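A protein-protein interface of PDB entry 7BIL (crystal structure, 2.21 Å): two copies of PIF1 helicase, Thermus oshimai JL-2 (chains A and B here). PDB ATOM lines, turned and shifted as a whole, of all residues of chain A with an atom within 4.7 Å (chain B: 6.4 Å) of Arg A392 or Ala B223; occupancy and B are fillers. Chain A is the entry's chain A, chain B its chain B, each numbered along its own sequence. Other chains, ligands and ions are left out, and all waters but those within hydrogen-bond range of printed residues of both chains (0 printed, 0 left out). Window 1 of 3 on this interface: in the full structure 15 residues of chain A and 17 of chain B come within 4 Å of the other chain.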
ATOM      1  N   TYR A 362      18.151  10.485 -17.593  1.00  0.00           N
ATOM      2  CA  TYR A 362      19.023  11.589 -17.947  1.00  0.00           C
ATOM      3  C   TYR A 362      18.273  12.563 -18.837  1.00  0.00           C
ATOM      4  O   TYR A 362      17.282  12.212 -19.491  1.00  0.00           O
ATOM      5  CB  TYR A 362      20.298  11.093 -18.632  1.00  0.00           C
ATOM      6  CG  TYR A 362      20.084  10.372 -19.942  1.00  0.00           C
ATOM      7  CD1 TYR A 362      19.959  11.072 -21.131  1.00  0.00           C
ATOM      8  CD2 TYR A 362      20.055   8.990 -19.997  1.00  0.00           C
ATOM      9  CE1 TYR A 362      19.787  10.405 -22.355  1.00  0.00           C
ATOM     10  CE2 TYR A 362      19.894   8.320 -21.204  1.00  0.00           C
ATOM     11  CZ  TYR A 362      19.756   9.034 -22.383  1.00  0.00           C
ATOM     12  OH  TYR A 362      19.589   8.378 -23.591  1.00  0.00           O
ATOM     13  N   GLU A 376      27.055   0.398 -30.022  1.00  0.00           N
ATOM     14  CA  GLU A 376      26.027   1.415 -30.213  1.00  0.00           C
ATOM     15  C   GLU A 376      25.517   1.921 -28.877  1.00  0.00           C
ATOM     16  O   GLU A 376      24.369   2.355 -28.761  1.00  0.00           O
ATOM     17  CB  GLU A 376      24.867   0.887 -31.057  1.00  0.00           C
ATOM     18  CG  GLU A 376      25.042   1.058 -32.565  1.00  0.00           C
ATOM     19  CD  GLU A 376      23.706   1.242 -33.288  1.00  0.00           C
ATOM     20  OE1 GLU A 376      22.657   0.841 -32.734  1.00  0.00           O
ATOM     21  OE2 GLU A 376      23.706   1.812 -34.401  1.00  0.00           O
ATOM     22  N   ALA A 377      26.376   1.884 -27.866  1.00  0.00           N
ATOM     23  CA  ALA A 377      25.949   2.134 -26.506  1.00  0.00           C
ATOM     24  C   ALA A 377      27.156   2.583 -25.696  1.00  0.00           C
ATOM     25  O   ALA A 377      28.241   2.013 -25.827  1.00  0.00           O
ATOM     26  CB  ALA A 377      25.340   0.850 -25.912  1.00  0.00           C
ATOM     27  N   VAL A 390      22.967   4.543 -19.465  1.00  0.00           N
ATOM     28  CA  VAL A 390      23.368   3.957 -20.737  1.00  0.00           C
ATOM     29  C   VAL A 390      22.770   4.762 -21.893  1.00  0.00           C
ATOM     30  O   VAL A 390      21.565   5.007 -21.929  1.00  0.00           O
ATOM     31  CB  VAL A 390      22.973   2.483 -20.824  1.00  0.00           C
ATOM     32  CG1 VAL A 390      23.299   1.972 -22.201  1.00  0.00           C
ATOM     33  CG2 VAL A 390      23.717   1.710 -19.766  1.00  0.00           C
ATOM     34  N   ILE A 391      23.634   5.257 -22.788  1.00  0.00           N
ATOM     35  CA  ILE A 391      23.274   6.153 -23.890  1.00  0.00           C
ATOM     36  C   ILE A 391      23.186   5.367 -25.198  1.00  0.00           C
ATOM     37  O   ILE A 391      24.117   4.634 -25.556  1.00  0.00           O
ATOM     38  CB  ILE A 391      24.301   7.294 -24.015  1.00  0.00           C
ATOM     39  CG1 ILE A 391      24.523   7.978 -22.667  1.00  0.00           C
ATOM     40  CG2 ILE A 391      23.863   8.312 -25.041  1.00  0.00           C
ATOM     41  CD1 ILE A 391      23.289   8.546 -22.067  1.00  0.00           C
ATOM     42  N   ARG A 392      22.068   5.486 -25.900  1.00  0.00           N
ATOM     43  CA  ARG A 392      21.920   4.866 -27.220  1.00  0.00           C
ATOM     44  C   ARG A 392      21.619   5.912 -28.296  1.00  0.00           C
ATOM     45  O   ARG A 392      21.344   7.061 -27.956  1.00  0.00           O
ATOM     46  CB  ARG A 392      20.854   3.779 -27.163  1.00  0.00           C
ATOM     47  CG  ARG A 392      21.320   2.575 -26.388  1.00  0.00           C
ATOM     48  CD  ARG A 392      20.543   1.338 -26.816  1.00  0.00           C
ATOM     49  NE  ARG A 392      19.154   1.435 -26.426  1.00  0.00           N
ATOM     50  CZ  ARG A 392      18.239   0.525 -26.733  1.00  0.00           C
ATOM     51  NH1 ARG A 392      18.584  -0.544 -27.445  1.00  0.00           N
ATOM     52  NH2 ARG A 392      16.989   0.689 -26.328  1.00  0.00           N
ATOM     53  N   PRO A 393      21.705   5.584 -29.588  1.00  0.00           N
ATOM     54  CA  PRO A 393      21.510   6.609 -30.627  1.00  0.00           C
ATOM     55  C   PRO A 393      20.082   7.147 -30.673  1.00  0.00           C
ATOM     56  O   PRO A 393      19.121   6.421 -30.437  1.00  0.00           O
ATOM     57  CB  PRO A 393      21.855   5.876 -31.929  1.00  0.00           C
ATOM     58  CG  PRO A 393      22.527   4.625 -31.522  1.00  0.00           C
ATOM     59  CD  PRO A 393      21.981   4.265 -30.195  1.00  0.00           C
ATOM     60  N   PHE A 394      19.962   8.446 -30.944  1.00  0.00           N
ATOM     61  CA  PHE A 394      18.701   9.149 -31.141  1.00  0.00           C
ATOM     62  C   PHE A 394      18.634   9.636 -32.581  1.00  0.00           C
ATOM     63  O   PHE A 394      19.639   9.687 -33.287  1.00  0.00           O
ATOM     64  CB  PHE A 394      18.568  10.364 -30.215  1.00  0.00           C
ATOM     65  CG  PHE A 394      18.072  10.060 -28.820  1.00  0.00           C
ATOM     66  CD1 PHE A 394      18.907   9.481 -27.870  1.00  0.00           C
ATOM     67  CD2 PHE A 394      16.797  10.432 -28.433  1.00  0.00           C
ATOM     68  CE1 PHE A 394      18.472   9.252 -26.583  1.00  0.00           C
ATOM     69  CE2 PHE A 394      16.360  10.192 -27.149  1.00  0.00           C
ATOM     70  CZ  PHE A 394      17.197   9.605 -26.227  1.00  0.00           C
ATOM     71  N   VAL A 421      24.544   8.984 -31.409  1.00  0.00           N
ATOM     72  CA  VAL A 421      24.555   9.010 -29.944  1.00  0.00           C
ATOM     73  C   VAL A 421      24.448  10.460 -29.460  1.00  0.00           C
ATOM     74  O   VAL A 421      25.214  11.331 -29.932  1.00  0.00           O
ATOM     75  CB  VAL A 421      25.841   8.328 -29.444  1.00  0.00           C
ATOM     76  CG1 VAL A 421      26.294   8.916 -28.177  1.00  0.00           C
ATOM     77  CG2 VAL A 421      25.602   6.823 -29.281  1.00  0.00           C
ATOM     78  N   PRO A 422      23.480  10.793 -28.566  1.00  0.00           N
ATOM     79  CA  PRO A 422      23.214  12.188 -28.158  1.00  0.00           C
ATOM     80  C   PRO A 422      24.227  12.737 -27.163  1.00  0.00           C
ATOM     81  O   PRO A 422      23.900  13.064 -26.019  1.00  0.00           O
ATOM     82  CB  PRO A 422      21.816  12.084 -27.553  1.00  0.00           C
ATOM     83  CG  PRO A 422      21.821  10.717 -26.949  1.00  0.00           C
ATOM     84  CD  PRO A 422      22.477   9.873 -27.979  1.00  0.00           C
ATOM     85  N   VAL B 217      15.343  -4.803 -28.284  1.00  0.00           N
ATOM     86  CA  VAL B 217      16.405  -4.500 -27.325  1.00  0.00           C
ATOM     87  C   VAL B 217      15.972  -3.350 -26.418  1.00  0.00           C
ATOM     88  O   VAL B 217      15.923  -2.199 -26.875  1.00  0.00           O
ATOM     89  CB  VAL B 217      17.733  -4.145 -28.024  1.00  0.00           C
ATOM     90  CG1 VAL B 217      18.815  -3.873 -26.978  1.00  0.00           C
ATOM     91  CG2 VAL B 217      18.175  -5.251 -28.993  1.00  0.00           C
ATOM     92  N   PRO B 218      15.651  -3.606 -25.155  1.00  0.00           N
ATOM     93  CA  PRO B 218      15.349  -2.514 -24.222  1.00  0.00           C
ATOM     94  C   PRO B 218      16.618  -1.787 -23.787  1.00  0.00           C
ATOM     95  O   PRO B 218      17.726  -2.313 -23.861  1.00  0.00           O
ATOM     96  CB  PRO B 218      14.696  -3.225 -23.024  1.00  0.00           C
ATOM     97  CG  PRO B 218      14.611  -4.723 -23.421  1.00  0.00           C
ATOM     98  CD  PRO B 218      15.658  -4.915 -24.488  1.00  0.00           C
ATOM     99  N   GLY B 219      16.442  -0.541 -23.354  1.00  0.00           N
ATOM    100  CA  GLY B 219      17.568   0.269 -22.923  1.00  0.00           C
ATOM    101  C   GLY B 219      18.254  -0.153 -21.635  1.00  0.00           C
ATOM    102  O   GLY B 219      18.103  -1.286 -21.166  1.00  0.00           O
ATOM    103  N   GLY B 220      19.034   0.759 -21.063  1.00  0.00           N
ATOM    104  CA  GLY B 220      19.750   0.505 -19.835  1.00  0.00           C
ATOM    105  C   GLY B 220      20.866  -0.513 -20.046  1.00  0.00           C
ATOM    106  O   GLY B 220      21.309  -0.789 -21.167  1.00  0.00           O
ATOM    107  N   GLU B 221      21.305  -1.088 -18.923  1.00  0.00           N
ATOM    108  CA  GLU B 221      22.479  -1.965 -18.894  1.00  0.00           C
ATOM    109  C   GLU B 221      22.343  -3.185 -19.798  1.00  0.00           C
ATOM    110  O   GLU B 221      23.358  -3.768 -20.218  1.00  0.00           O
ATOM    111  CB  GLU B 221      22.760  -2.378 -17.451  1.00  0.00           C
ATOM    112  CG  GLU B 221      23.052  -1.178 -16.527  1.00  0.00           C
ATOM    113  CD  GLU B 221      24.453  -0.599 -16.738  1.00  0.00           C
ATOM    114  OE1 GLU B 221      24.753   0.493 -16.205  1.00  0.00           O
ATOM    115  OE2 GLU B 221      25.260  -1.248 -17.433  1.00  0.00           O
ATOM    116  N   GLU B 222      21.108  -3.603 -20.079  1.00  0.00           N
ATOM    117  CA  GLU B 222      20.874  -4.759 -20.934  1.00  0.00           C
ATOM    118  C   GLU B 222      21.362  -4.488 -22.362  1.00  0.00           C
ATOM    119  O   GLU B 222      22.042  -5.326 -22.979  1.00  0.00           O
ATOM    120  CB  GLU B 222      19.383  -5.118 -20.886  1.00  0.00           C
ATOM    121  CG  GLU B 222      18.944  -6.169 -21.881  1.00  0.00           C
ATOM    122  CD  GLU B 222      17.468  -6.566 -21.704  1.00  0.00           C
ATOM    123  OE1 GLU B 222      16.792  -5.958 -20.840  1.00  0.00           O
ATOM    124  OE2 GLU B 222      16.993  -7.486 -22.420  1.00  0.00           O
ATOM    125  N   ALA B 223      21.047  -3.309 -22.894  1.00  0.00           N
ATOM    126  CA  ALA B 223      21.542  -2.939 -24.217  1.00  0.00           C
ATOM    127  C   ALA B 223      23.061  -2.862 -24.223  1.00  0.00           C
ATOM    128  O   ALA B 223      23.706  -3.300 -25.181  1.00  0.00           O
ATOM    129  CB  ALA B 223      20.957  -1.594 -24.644  1.00  0.00           C
ATOM    130  N   LEU B 224      23.652  -2.344 -23.141  1.00  0.00           N
ATOM    131  CA  LEU B 224      25.106  -2.209 -23.096  1.00  0.00           C
ATOM    132  C   LEU B 224      25.774  -3.570 -23.074  1.00  0.00           C
ATOM    133  O   LEU B 224      26.818  -3.759 -23.708  1.00  0.00           O
ATOM    134  CB  LEU B 224      25.544  -1.411 -21.862  1.00  0.00           C
ATOM    135  CG  LEU B 224      27.036  -1.074 -21.764  1.00  0.00           C
ATOM    136  CD1 LEU B 224      27.395  -0.056 -22.801  1.00  0.00           C
ATOM    137  CD2 LEU B 224      27.408  -0.544 -20.408  1.00  0.00           C
ATOM    138  N   TYR B 225      25.191  -4.528 -22.342  1.00  0.00           N
ATOM    139  CA  TYR B 225      25.787  -5.857 -22.247  1.00  0.00           C
ATOM    140  C   TYR B 225      25.785  -6.558 -23.601  1.00  0.00           C
ATOM    141  O   TYR B 225      26.748  -7.261 -23.956  1.00  0.00           O
ATOM    142  CB  TYR B 225      25.051  -6.704 -21.203  1.00  0.00           C
ATOM    143  CG  TYR B 225      25.551  -8.138 -21.157  1.00  0.00           C
ATOM    144  CD1 TYR B 225      26.660  -8.478 -20.386  1.00  0.00           C
ATOM    145  CD2 TYR B 225      24.943  -9.138 -21.923  1.00  0.00           C
ATOM    146  CE1 TYR B 225      27.139  -9.773 -20.354  1.00  0.00           C
ATOM    147  CE2 TYR B 225      25.420 -10.440 -21.900  1.00  0.00           C
ATOM    148  CZ  TYR B 225      26.519 -10.748 -21.112  1.00  0.00           C
ATOM    149  OH  TYR B 225      26.993 -12.035 -21.088  1.00  0.00           O
ATOM    150  N   ILE B 226      24.706  -6.384 -24.364  1.00  0.00           N
ATOM    151  CA  ILE B 226      24.620  -6.992 -25.684  1.00  0.00           C
ATOM    152  C   ILE B 226      25.680  -6.402 -26.611  1.00  0.00           C
ATOM    153  O   ILE B 226      26.369  -7.137 -27.334  1.00  0.00           O
ATOM    154  CB  ILE B 226      23.201  -6.842 -26.250  1.00  0.00           C
ATOM    155  CG1 ILE B 226      22.222  -7.648 -25.401  1.00  0.00           C
ATOM    156  CG2 ILE B 226      23.180  -7.288 -27.708  1.00  0.00           C
ATOM    157  CD1 ILE B 226      20.783  -7.576 -25.893  1.00  0.00           C
ATOM    158  N   ALA B 227      25.863  -5.073 -26.567  1.00  0.00           N
ATOM    159  CA  ALA B 227      26.860  -4.425 -27.419  1.00  0.00           C
ATOM    160  C   ALA B 227      28.264  -4.874 -27.052  1.00  0.00           C
ATOM    161  O   ALA B 227      29.085  -5.153 -27.931  1.00  0.00           O
ATOM    162  CB  ALA B 227      26.763  -2.906 -27.287  1.00  0.00           C
ATOM    163  N   ARG B 228      28.530  -5.035 -25.759  1.00  0.00           N
ATOM    164  CA  ARG B 228      29.864  -5.430 -25.314  1.00  0.00           C
ATOM    165  C   ARG B 228      30.126  -6.896 -25.643  1.00  0.00           C
ATOM    166  O   ARG B 228      31.251  -7.264 -25.998  1.00  0.00           O
ATOM    167  CB  ARG B 228      30.025  -5.158 -23.812  1.00  0.00           C
ATOM    168  CG  ARG B 228      31.237  -5.804 -23.136  1.00  0.00           C
ATOM    169  CD  ARG B 228      31.350  -5.456 -21.625  1.00  0.00           C
ATOM    170  NE  ARG B 228      30.089  -5.601 -20.887  1.00  0.00           N
ATOM    171  CZ  ARG B 228      29.405  -4.590 -20.342  1.00  0.00           C
ATOM    172  NH1 ARG B 228      29.876  -3.338 -20.433  1.00  0.00           N
ATOM    173  NH2 ARG B 228      28.258  -4.828 -19.693  1.00  0.00           N
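Arg A392 touches four residues of chain B.
Of the printed residues of chain A, Val B217 touches Arg A392.
Of the printed residues of chain A, Pro B218 touches Arg A392.
Of the printed residues of chain A, Gly B219 touches Arg A392.
Of the printed residues of chain A, Gly B220 touches Val A390 (3.6 Å).
Of the printed residues of chain A, Leu B224 touches Ala A377.
The nearest residue of chain B that does not touch Arg A392 is Gly B220 (5.4 Å).
The guanidinium group of Arg A392 lies close to the backbone NH of Gly B219.
The backbone carbonyl oxygen of Val B217 sits at hydrogen-bond distance from the guanidinium group of Arg A392.
Printed residues of chain A that touch a printed residue of chain B: Ala A377, Val A390 and Arg A392.
Hydrophobic or aromatic side chains of chain A within 4 Å of the printed part of chain B: Ala A377 and Val A390.
Among the printed residues, no Asp or Glu carboxylate lies within 4 Å of a Lys or Arg side-chain nitrogen of the other chain.
Among the printed residues, pairs that only touch across the chains: Val A390 with Gly B220 (3.6 Å), Arg A392 with Pro B218 (3.6 Å), Arg A392 with Ala B223 (3.7 Å), Ala A377 with Leu B224 (3.8 Å) and Val A390 with Glu B221 (3.8 Å).
No position is printed for both chains.
Of the 7 pairs that touch across the chains among the printed residues, none has its exchanged pair printed and touching as well.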
